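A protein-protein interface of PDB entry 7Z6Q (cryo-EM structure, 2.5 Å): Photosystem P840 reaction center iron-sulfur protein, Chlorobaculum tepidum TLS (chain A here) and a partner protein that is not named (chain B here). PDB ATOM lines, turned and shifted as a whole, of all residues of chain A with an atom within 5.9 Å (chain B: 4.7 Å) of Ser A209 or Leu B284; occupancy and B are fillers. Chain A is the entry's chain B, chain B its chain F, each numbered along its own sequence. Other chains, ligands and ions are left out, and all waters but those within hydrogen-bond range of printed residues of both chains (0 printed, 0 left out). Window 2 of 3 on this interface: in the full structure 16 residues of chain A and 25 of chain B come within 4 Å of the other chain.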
ATOM      1  N   PHE A 186     -15.126 -31.490  -1.185  1.00  0.00           N
ATOM      2  CA  PHE A 186     -16.170 -30.862  -2.037  1.00  0.00           C
ATOM      3  C   PHE A 186     -17.015 -29.811  -1.299  1.00  0.00           C
ATOM      4  O   PHE A 186     -17.254 -28.737  -1.891  1.00  0.00           O
ATOM      5  CB  PHE A 186     -17.033 -31.920  -2.728  1.00  0.00           C
ATOM      6  CG  PHE A 186     -17.850 -31.357  -3.860  1.00  0.00           C
ATOM      7  CD1 PHE A 186     -17.237 -30.911  -5.017  1.00  0.00           C
ATOM      8  CD2 PHE A 186     -19.221 -31.222  -3.745  1.00  0.00           C
ATOM      9  CE1 PHE A 186     -17.985 -30.368  -6.048  1.00  0.00           C
ATOM     10  CE2 PHE A 186     -19.966 -30.679  -4.780  1.00  0.00           C
ATOM     11  CZ  PHE A 186     -19.348 -30.256  -5.930  1.00  0.00           C
ATOM     12  N   SER A 187     -17.441 -30.124  -0.067  1.00  0.00           N
ATOM     13  CA  SER A 187     -18.341 -29.264   0.753  1.00  0.00           C
ATOM     14  C   SER A 187     -17.900 -27.800   0.775  1.00  0.00           C
ATOM     15  O   SER A 187     -18.703 -26.930   0.403  1.00  0.00           O
ATOM     16  CB  SER A 187     -18.425 -29.769   2.162  1.00  0.00           C
ATOM     17  OG  SER A 187     -19.358 -30.828   2.259  1.00  0.00           O
ATOM     18  N   GLY A 188     -16.666 -27.565   1.223  1.00  0.00           N
ATOM     19  CA  GLY A 188     -16.036 -26.262   1.201  1.00  0.00           C
ATOM     20  C   GLY A 188     -15.690 -25.938  -0.236  1.00  0.00           C
ATOM     21  O   GLY A 188     -14.987 -26.717  -0.901  1.00  0.00           O
ATOM     22  N   ASP A 189     -16.163 -24.799  -0.733  1.00  0.00           N
ATOM     23  CA  ASP A 189     -15.987 -24.461  -2.140  1.00  0.00           C
ATOM     24  C   ASP A 189     -14.557 -23.977  -2.333  1.00  0.00           C
ATOM     25  O   ASP A 189     -14.320 -22.790  -2.579  1.00  0.00           O
ATOM     26  CB  ASP A 189     -16.987 -23.381  -2.546  1.00  0.00           C
ATOM     27  CG  ASP A 189     -18.413 -23.888  -2.556  1.00  0.00           C
ATOM     28  OD1 ASP A 189     -18.613 -25.096  -2.799  1.00  0.00           O
ATOM     29  OD2 ASP A 189     -19.337 -23.080  -2.325  1.00  0.00           O
ATOM     30  N   LEU A 206     -21.149 -32.927 -10.634  1.00  0.00           N
ATOM     31  CA  LEU A 206     -21.226 -31.561 -10.136  1.00  0.00           C
ATOM     32  C   LEU A 206     -19.821 -30.984 -10.039  1.00  0.00           C
ATOM     33  O   LEU A 206     -18.970 -31.533  -9.333  1.00  0.00           O
ATOM     34  CB  LEU A 206     -21.904 -31.512  -8.769  1.00  0.00           C
ATOM     35  CG  LEU A 206     -23.426 -31.455  -8.684  1.00  0.00           C
ATOM     36  CD1 LEU A 206     -24.066 -32.729  -9.203  1.00  0.00           C
ATOM     37  CD2 LEU A 206     -23.812 -31.210  -7.250  1.00  0.00           C
ATOM     38  N   ASP A 207     -19.604 -29.846 -10.697  1.00  0.00           N
ATOM     39  CA  ASP A 207     -18.274 -29.187 -10.656  1.00  0.00           C
ATOM     40  C   ASP A 207     -18.205 -28.205  -9.481  1.00  0.00           C
ATOM     41  O   ASP A 207     -17.090 -27.944  -9.016  1.00  0.00           O
ATOM     42  CB  ASP A 207     -17.950 -28.500 -11.981  1.00  0.00           C
ATOM     43  CG  ASP A 207     -18.642 -27.165 -12.151  1.00  0.00           C
ATOM     44  OD1 ASP A 207     -19.756 -27.010 -11.617  1.00  0.00           O
ATOM     45  OD2 ASP A 207     -18.067 -26.299 -12.821  1.00  0.00           O
ATOM     46  N   PHE A 208     -19.350 -27.691  -9.025  1.00  0.00           N
ATOM     47  CA  PHE A 208     -19.402 -26.739  -7.928  1.00  0.00           C
ATOM     48  C   PHE A 208     -20.674 -26.983  -7.130  1.00  0.00           C
ATOM     49  O   PHE A 208     -21.672 -27.473  -7.664  1.00  0.00           O
ATOM     50  CB  PHE A 208     -19.356 -25.299  -8.461  1.00  0.00           C
ATOM     51  CG  PHE A 208     -18.960 -24.277  -7.438  1.00  0.00           C
ATOM     52  CD1 PHE A 208     -17.646 -24.171  -7.016  1.00  0.00           C
ATOM     53  CD2 PHE A 208     -19.892 -23.404  -6.917  1.00  0.00           C
ATOM     54  CE1 PHE A 208     -17.277 -23.221  -6.083  1.00  0.00           C
ATOM     55  CE2 PHE A 208     -19.533 -22.455  -5.986  1.00  0.00           C
ATOM     56  CZ  PHE A 208     -18.224 -22.362  -5.569  1.00  0.00           C
ATOM     57  N   SER A 209     -20.632 -26.638  -5.842  1.00  0.00           N
ATOM     58  CA  SER A 209     -21.722 -26.981  -4.936  1.00  0.00           C
ATOM     59  C   SER A 209     -23.011 -26.220  -5.228  1.00  0.00           C
ATOM     60  O   SER A 209     -24.095 -26.751  -4.967  1.00  0.00           O
ATOM     61  CB  SER A 209     -21.294 -26.739  -3.487  1.00  0.00           C
ATOM     62  OG  SER A 209     -20.243 -27.609  -3.113  1.00  0.00           O
ATOM     63  N   TYR A 210     -22.926 -24.997  -5.747  1.00  0.00           N
ATOM     64  CA  TYR A 210     -24.105 -24.277  -6.212  1.00  0.00           C
ATOM     65  C   TYR A 210     -23.704 -23.404  -7.391  1.00  0.00           C
ATOM     66  O   TYR A 210     -22.688 -22.711  -7.326  1.00  0.00           O
ATOM     67  CB  TYR A 210     -24.726 -23.408  -5.108  1.00  0.00           C
ATOM     68  CG  TYR A 210     -25.551 -22.271  -5.672  1.00  0.00           C
ATOM     69  CD1 TYR A 210     -26.834 -22.495  -6.153  1.00  0.00           C
ATOM     70  CD2 TYR A 210     -25.037 -20.984  -5.754  1.00  0.00           C
ATOM     71  CE1 TYR A 210     -27.584 -21.471  -6.687  1.00  0.00           C
ATOM     72  CE2 TYR A 210     -25.780 -19.954  -6.289  1.00  0.00           C
ATOM     73  CZ  TYR A 210     -27.053 -20.203  -6.753  1.00  0.00           C
ATOM     74  OH  TYR A 210     -27.799 -19.178  -7.283  1.00  0.00           O
ATOM     75  N   THR A 211     -24.514 -23.408  -8.445  1.00  0.00           N
ATOM     76  CA  THR A 211     -24.182 -22.636  -9.630  1.00  0.00           C
ATOM     77  C   THR A 211     -25.170 -21.497  -9.825  1.00  0.00           C
ATOM     78  O   THR A 211     -26.386 -21.726  -9.795  1.00  0.00           O
ATOM     79  CB  THR A 211     -24.168 -23.534 -10.873  1.00  0.00           C
ATOM     80  OG1 THR A 211     -23.365 -24.693 -10.615  1.00  0.00           O
ATOM     81  CG2 THR A 211     -23.593 -22.784 -12.065  1.00  0.00           C
ATOM     82  N   ASP B 279     -36.212 -32.859  -2.192  1.00  0.00           N
ATOM     83  CA  ASP B 279     -34.941 -32.912  -2.965  1.00  0.00           C
ATOM     84  C   ASP B 279     -35.006 -31.906  -4.120  1.00  0.00           C
ATOM     85  O   ASP B 279     -36.080 -31.793  -4.744  1.00  0.00           O
ATOM     86  CB  ASP B 279     -34.651 -34.331  -3.464  1.00  0.00           C
ATOM     87  CG  ASP B 279     -33.200 -34.550  -3.851  1.00  0.00           C
ATOM     88  OD1 ASP B 279     -32.317 -34.144  -3.069  1.00  0.00           O
ATOM     89  OD2 ASP B 279     -32.963 -35.123  -4.933  1.00  0.00           O
ATOM     90  N   ALA B 280     -33.895 -31.214  -4.390  1.00  0.00           N
ATOM     91  CA  ALA B 280     -33.844 -30.227  -5.455  1.00  0.00           C
ATOM     92  C   ALA B 280     -32.861 -30.589  -6.561  1.00  0.00           C
ATOM     93  O   ALA B 280     -32.758 -29.843  -7.542  1.00  0.00           O
ATOM     94  CB  ALA B 280     -33.481 -28.848  -4.884  1.00  0.00           C
ATOM     95  N   GLY B 281     -32.143 -31.695  -6.435  1.00  0.00           N
ATOM     96  CA  GLY B 281     -31.190 -32.115  -7.453  1.00  0.00           C
ATOM     97  C   GLY B 281     -29.764 -31.737  -7.110  1.00  0.00           C
ATOM     98  O   GLY B 281     -29.492 -30.727  -6.465  1.00  0.00           O
ATOM     99  N   GLY B 282     -28.833 -32.574  -7.559  1.00  0.00           N
ATOM    100  CA  GLY B 282     -27.424 -32.355  -7.273  1.00  0.00           C
ATOM    101  C   GLY B 282     -27.067 -32.434  -5.805  1.00  0.00           C
ATOM    102  O   GLY B 282     -26.179 -31.705  -5.347  1.00  0.00           O
ATOM    103  N   GLY B 283     -27.741 -33.304  -5.052  1.00  0.00           N
ATOM    104  CA  GLY B 283     -27.476 -33.463  -3.640  1.00  0.00           C
ATOM    105  C   GLY B 283     -27.997 -32.347  -2.768  1.00  0.00           C
ATOM    106  O   GLY B 283     -27.697 -32.329  -1.566  1.00  0.00           O
ATOM    107  N   LEU B 284     -28.707 -31.388  -3.369  1.00  0.00           N
ATOM    108  CA  LEU B 284     -29.178 -30.200  -2.607  1.00  0.00           C
ATOM    109  C   LEU B 284     -30.645 -30.341  -2.191  1.00  0.00           C
ATOM    110  O   LEU B 284     -31.461 -30.802  -3.014  1.00  0.00           O
ATOM    111  CB  LEU B 284     -28.970 -28.949  -3.468  1.00  0.00           C
ATOM    112  CG  LEU B 284     -27.579 -28.323  -3.394  1.00  0.00           C
ATOM    113  CD1 LEU B 284     -26.534 -29.256  -3.985  1.00  0.00           C
ATOM    114  CD2 LEU B 284     -27.551 -26.975  -4.100  1.00  0.00           C
ATOM    115  N   ARG B 285     -30.944 -29.951  -0.948  1.00  0.00           N
ATOM    116  CA  ARG B 285     -32.328 -29.962  -0.404  1.00  0.00           C
ATOM    117  C   ARG B 285     -32.921 -28.555  -0.576  1.00  0.00           C
ATOM    118  O   ARG B 285     -32.148 -27.614  -0.853  1.00  0.00           O
ATOM    119  CB  ARG B 285     -32.320 -30.380   1.070  1.00  0.00           C
ATOM    120  CG  ARG B 285     -32.065 -31.863   1.294  1.00  0.00           C
ATOM    121  CD  ARG B 285     -32.774 -32.391   2.527  1.00  0.00           C
ATOM    122  NE  ARG B 285     -34.219 -32.439   2.358  1.00  0.00           N
ATOM    123  CZ  ARG B 285     -34.880 -33.457   1.821  1.00  0.00           C
ATOM    124  NH1 ARG B 285     -34.223 -34.523   1.395  1.00  0.00           N
ATOM    125  NH2 ARG B 285     -36.196 -33.407   1.711  1.00  0.00           N
ATOM    126  N   ARG B 286     -34.238 -28.411  -0.409  1.00  0.00           N
ATOM    127  CA  ARG B 286     -34.867 -27.074  -0.589  1.00  0.00           C
ATOM    128  C   ARG B 286     -36.233 -27.035   0.107  1.00  0.00           C
ATOM    129  O   ARG B 286     -36.947 -28.049   0.038  1.00  0.00           O
ATOM    130  CB  ARG B 286     -35.049 -26.848  -2.096  1.00  0.00           C
ATOM    131  CG  ARG B 286     -36.035 -25.754  -2.481  1.00  0.00           C
ATOM    132  CD  ARG B 286     -36.885 -26.128  -3.677  1.00  0.00           C
ATOM    133  NE  ARG B 286     -36.167 -25.980  -4.932  1.00  0.00           N
ATOM    134  CZ  ARG B 286     -36.468 -26.634  -6.046  1.00  0.00           C
ATOM    135  NH1 ARG B 286     -37.473 -27.494  -6.055  1.00  0.00           N
ATOM    136  NH2 ARG B 286     -35.758 -26.435  -7.142  1.00  0.00           N
ATOM    137  N   ARG B 324     -26.812 -23.011   0.368  1.00  0.00           N
ATOM    138  CA  ARG B 324     -25.928 -22.774  -0.802  1.00  0.00           C
ATOM    139  C   ARG B 324     -26.405 -21.508  -1.522  1.00  0.00           C
ATOM    140  O   ARG B 324     -25.552 -20.805  -2.102  1.00  0.00           O
ATOM    141  CB  ARG B 324     -25.946 -23.985  -1.738  1.00  0.00           C
ATOM    142  CG  ARG B 324     -25.291 -25.231  -1.158  1.00  0.00           C
ATOM    143  CD  ARG B 324     -23.952 -24.926  -0.511  1.00  0.00           C
ATOM    144  NE  ARG B 324     -23.286 -26.123  -0.021  1.00  0.00           N
ATOM    145  CZ  ARG B 324     -22.168 -26.123   0.695  1.00  0.00           C
ATOM    146  NH1 ARG B 324     -21.637 -27.265   1.097  1.00  0.00           N
ATOM    147  NH2 ARG B 324     -21.584 -24.980   1.009  1.00  0.00           N
ATOM    148  N   LEU B 363     -31.733 -23.084  -0.797  1.00  0.00           N
ATOM    149  CA  LEU B 363     -31.114 -24.399  -1.088  1.00  0.00           C
ATOM    150  C   LEU B 363     -30.100 -24.660   0.022  1.00  0.00           C
ATOM    151  O   LEU B 363     -29.163 -23.864   0.149  1.00  0.00           O
ATOM    152  CB  LEU B 363     -30.387 -24.324  -2.433  1.00  0.00           C
ATOM    153  CG  LEU B 363     -31.260 -24.101  -3.664  1.00  0.00           C
ATOM    154  CD1 LEU B 363     -30.416 -24.085  -4.927  1.00  0.00           C
ATOM    155  CD2 LEU B 363     -32.347 -25.155  -3.758  1.00  0.00           C
ATOM    156  N   TYR B 364     -30.270 -25.731   0.789  1.00  0.00           N
ATOM    157  CA  TYR B 364     -29.288 -26.019   1.863  1.00  0.00           C
ATOM    158  C   TYR B 364     -28.699 -27.404   1.618  1.00  0.00           C
ATOM    159  O   TYR B 364     -29.455 -28.383   1.582  1.00  0.00           O
ATOM    160  CB  TYR B 364     -29.960 -25.942   3.234  1.00  0.00           C
ATOM    161  CG  TYR B 364     -31.093 -26.917   3.427  1.00  0.00           C
ATOM    162  CD1 TYR B 364     -32.387 -26.588   3.062  1.00  0.00           C
ATOM    163  CD2 TYR B 364     -30.868 -28.169   3.973  1.00  0.00           C
ATOM    164  CE1 TYR B 364     -33.429 -27.479   3.237  1.00  0.00           C
ATOM    165  CE2 TYR B 364     -31.901 -29.069   4.158  1.00  0.00           C
ATOM    166  CZ  TYR B 364     -33.185 -28.724   3.788  1.00  0.00           C
ATOM    167  OH  TYR B 364     -34.205 -29.609   3.964  1.00  0.00           O
ATOM    168  N   ALA B 365     -27.378 -27.484   1.488  1.00  0.00           N
ATOM    169  CA  ALA B 365     -26.744 -28.794   1.249  1.00  0.00           C
ATOM    170  C   ALA B 365     -25.887 -29.151   2.459  1.00  0.00           C
ATOM    171  O   ALA B 365     -25.482 -28.237   3.189  1.00  0.00           O
ATOM    172  CB  ALA B 365     -25.909 -28.740  -0.004  1.00  0.00           C
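The backbone carbonyl oxygen of Ser A187 lies within hydrogen-bond range of the guanidinium group of Arg B324, 3.0 Å away.
Printed residues of chain B within 4 Å of Leu A206: Gly B282 (3.1 Å).
Of the printed residues of chain B, Ser A209 touches Leu B284 (3.6 Å).
Of the printed residues of chain B, Tyr A210 touches Arg B324 (3.6 Å).
Leu B284 touches one residue of chain A.
Printed residues of chain A within 4 Å of Arg B324: Ser A187 (3.0 Å) and Tyr A210 (3.6 Å).
Ala B365 touches none of the printed residues of chain A.
The nearest printed residue of chain B that does not touch Ser A187 is Ala B365 (6.7 Å).
Leu A206 touches Gly B282.
Ser A209 touches Leu B284.
CB of Arg B324 touches CB of Tyr A210 (3.6 Å).
Of the 12 printed residues of chain B, 3 touch a printed residue of chain A.
Printed residues of chain B that touch a printed residue of chain A: Gly B282, Leu B284 and Arg B324.
Hydrophobic or aromatic side chains of chain B within 4 Å of the printed part of chain A: Leu B284.
Of the 10 printed residues of chain A, 4 touch a printed residue of chain B.
Among the printed residues, 4 pairs touch across the chains.
Among the printed residues, no Asp or Glu carboxylate lies within 4 Å of a Lys or Arg side-chain nitrogen of the other chain.
OG of Ser A209 sits at hydrogen-bond distance from O of Phe A186 (3.4 Å).
N of Arg B324 lies within hydrogen-bond range of O of Leu B363 (2.5 Å).
OD1 of Asp A189 sits at hydrogen-bond distance from OG of Ser A209 (3.0 Å).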
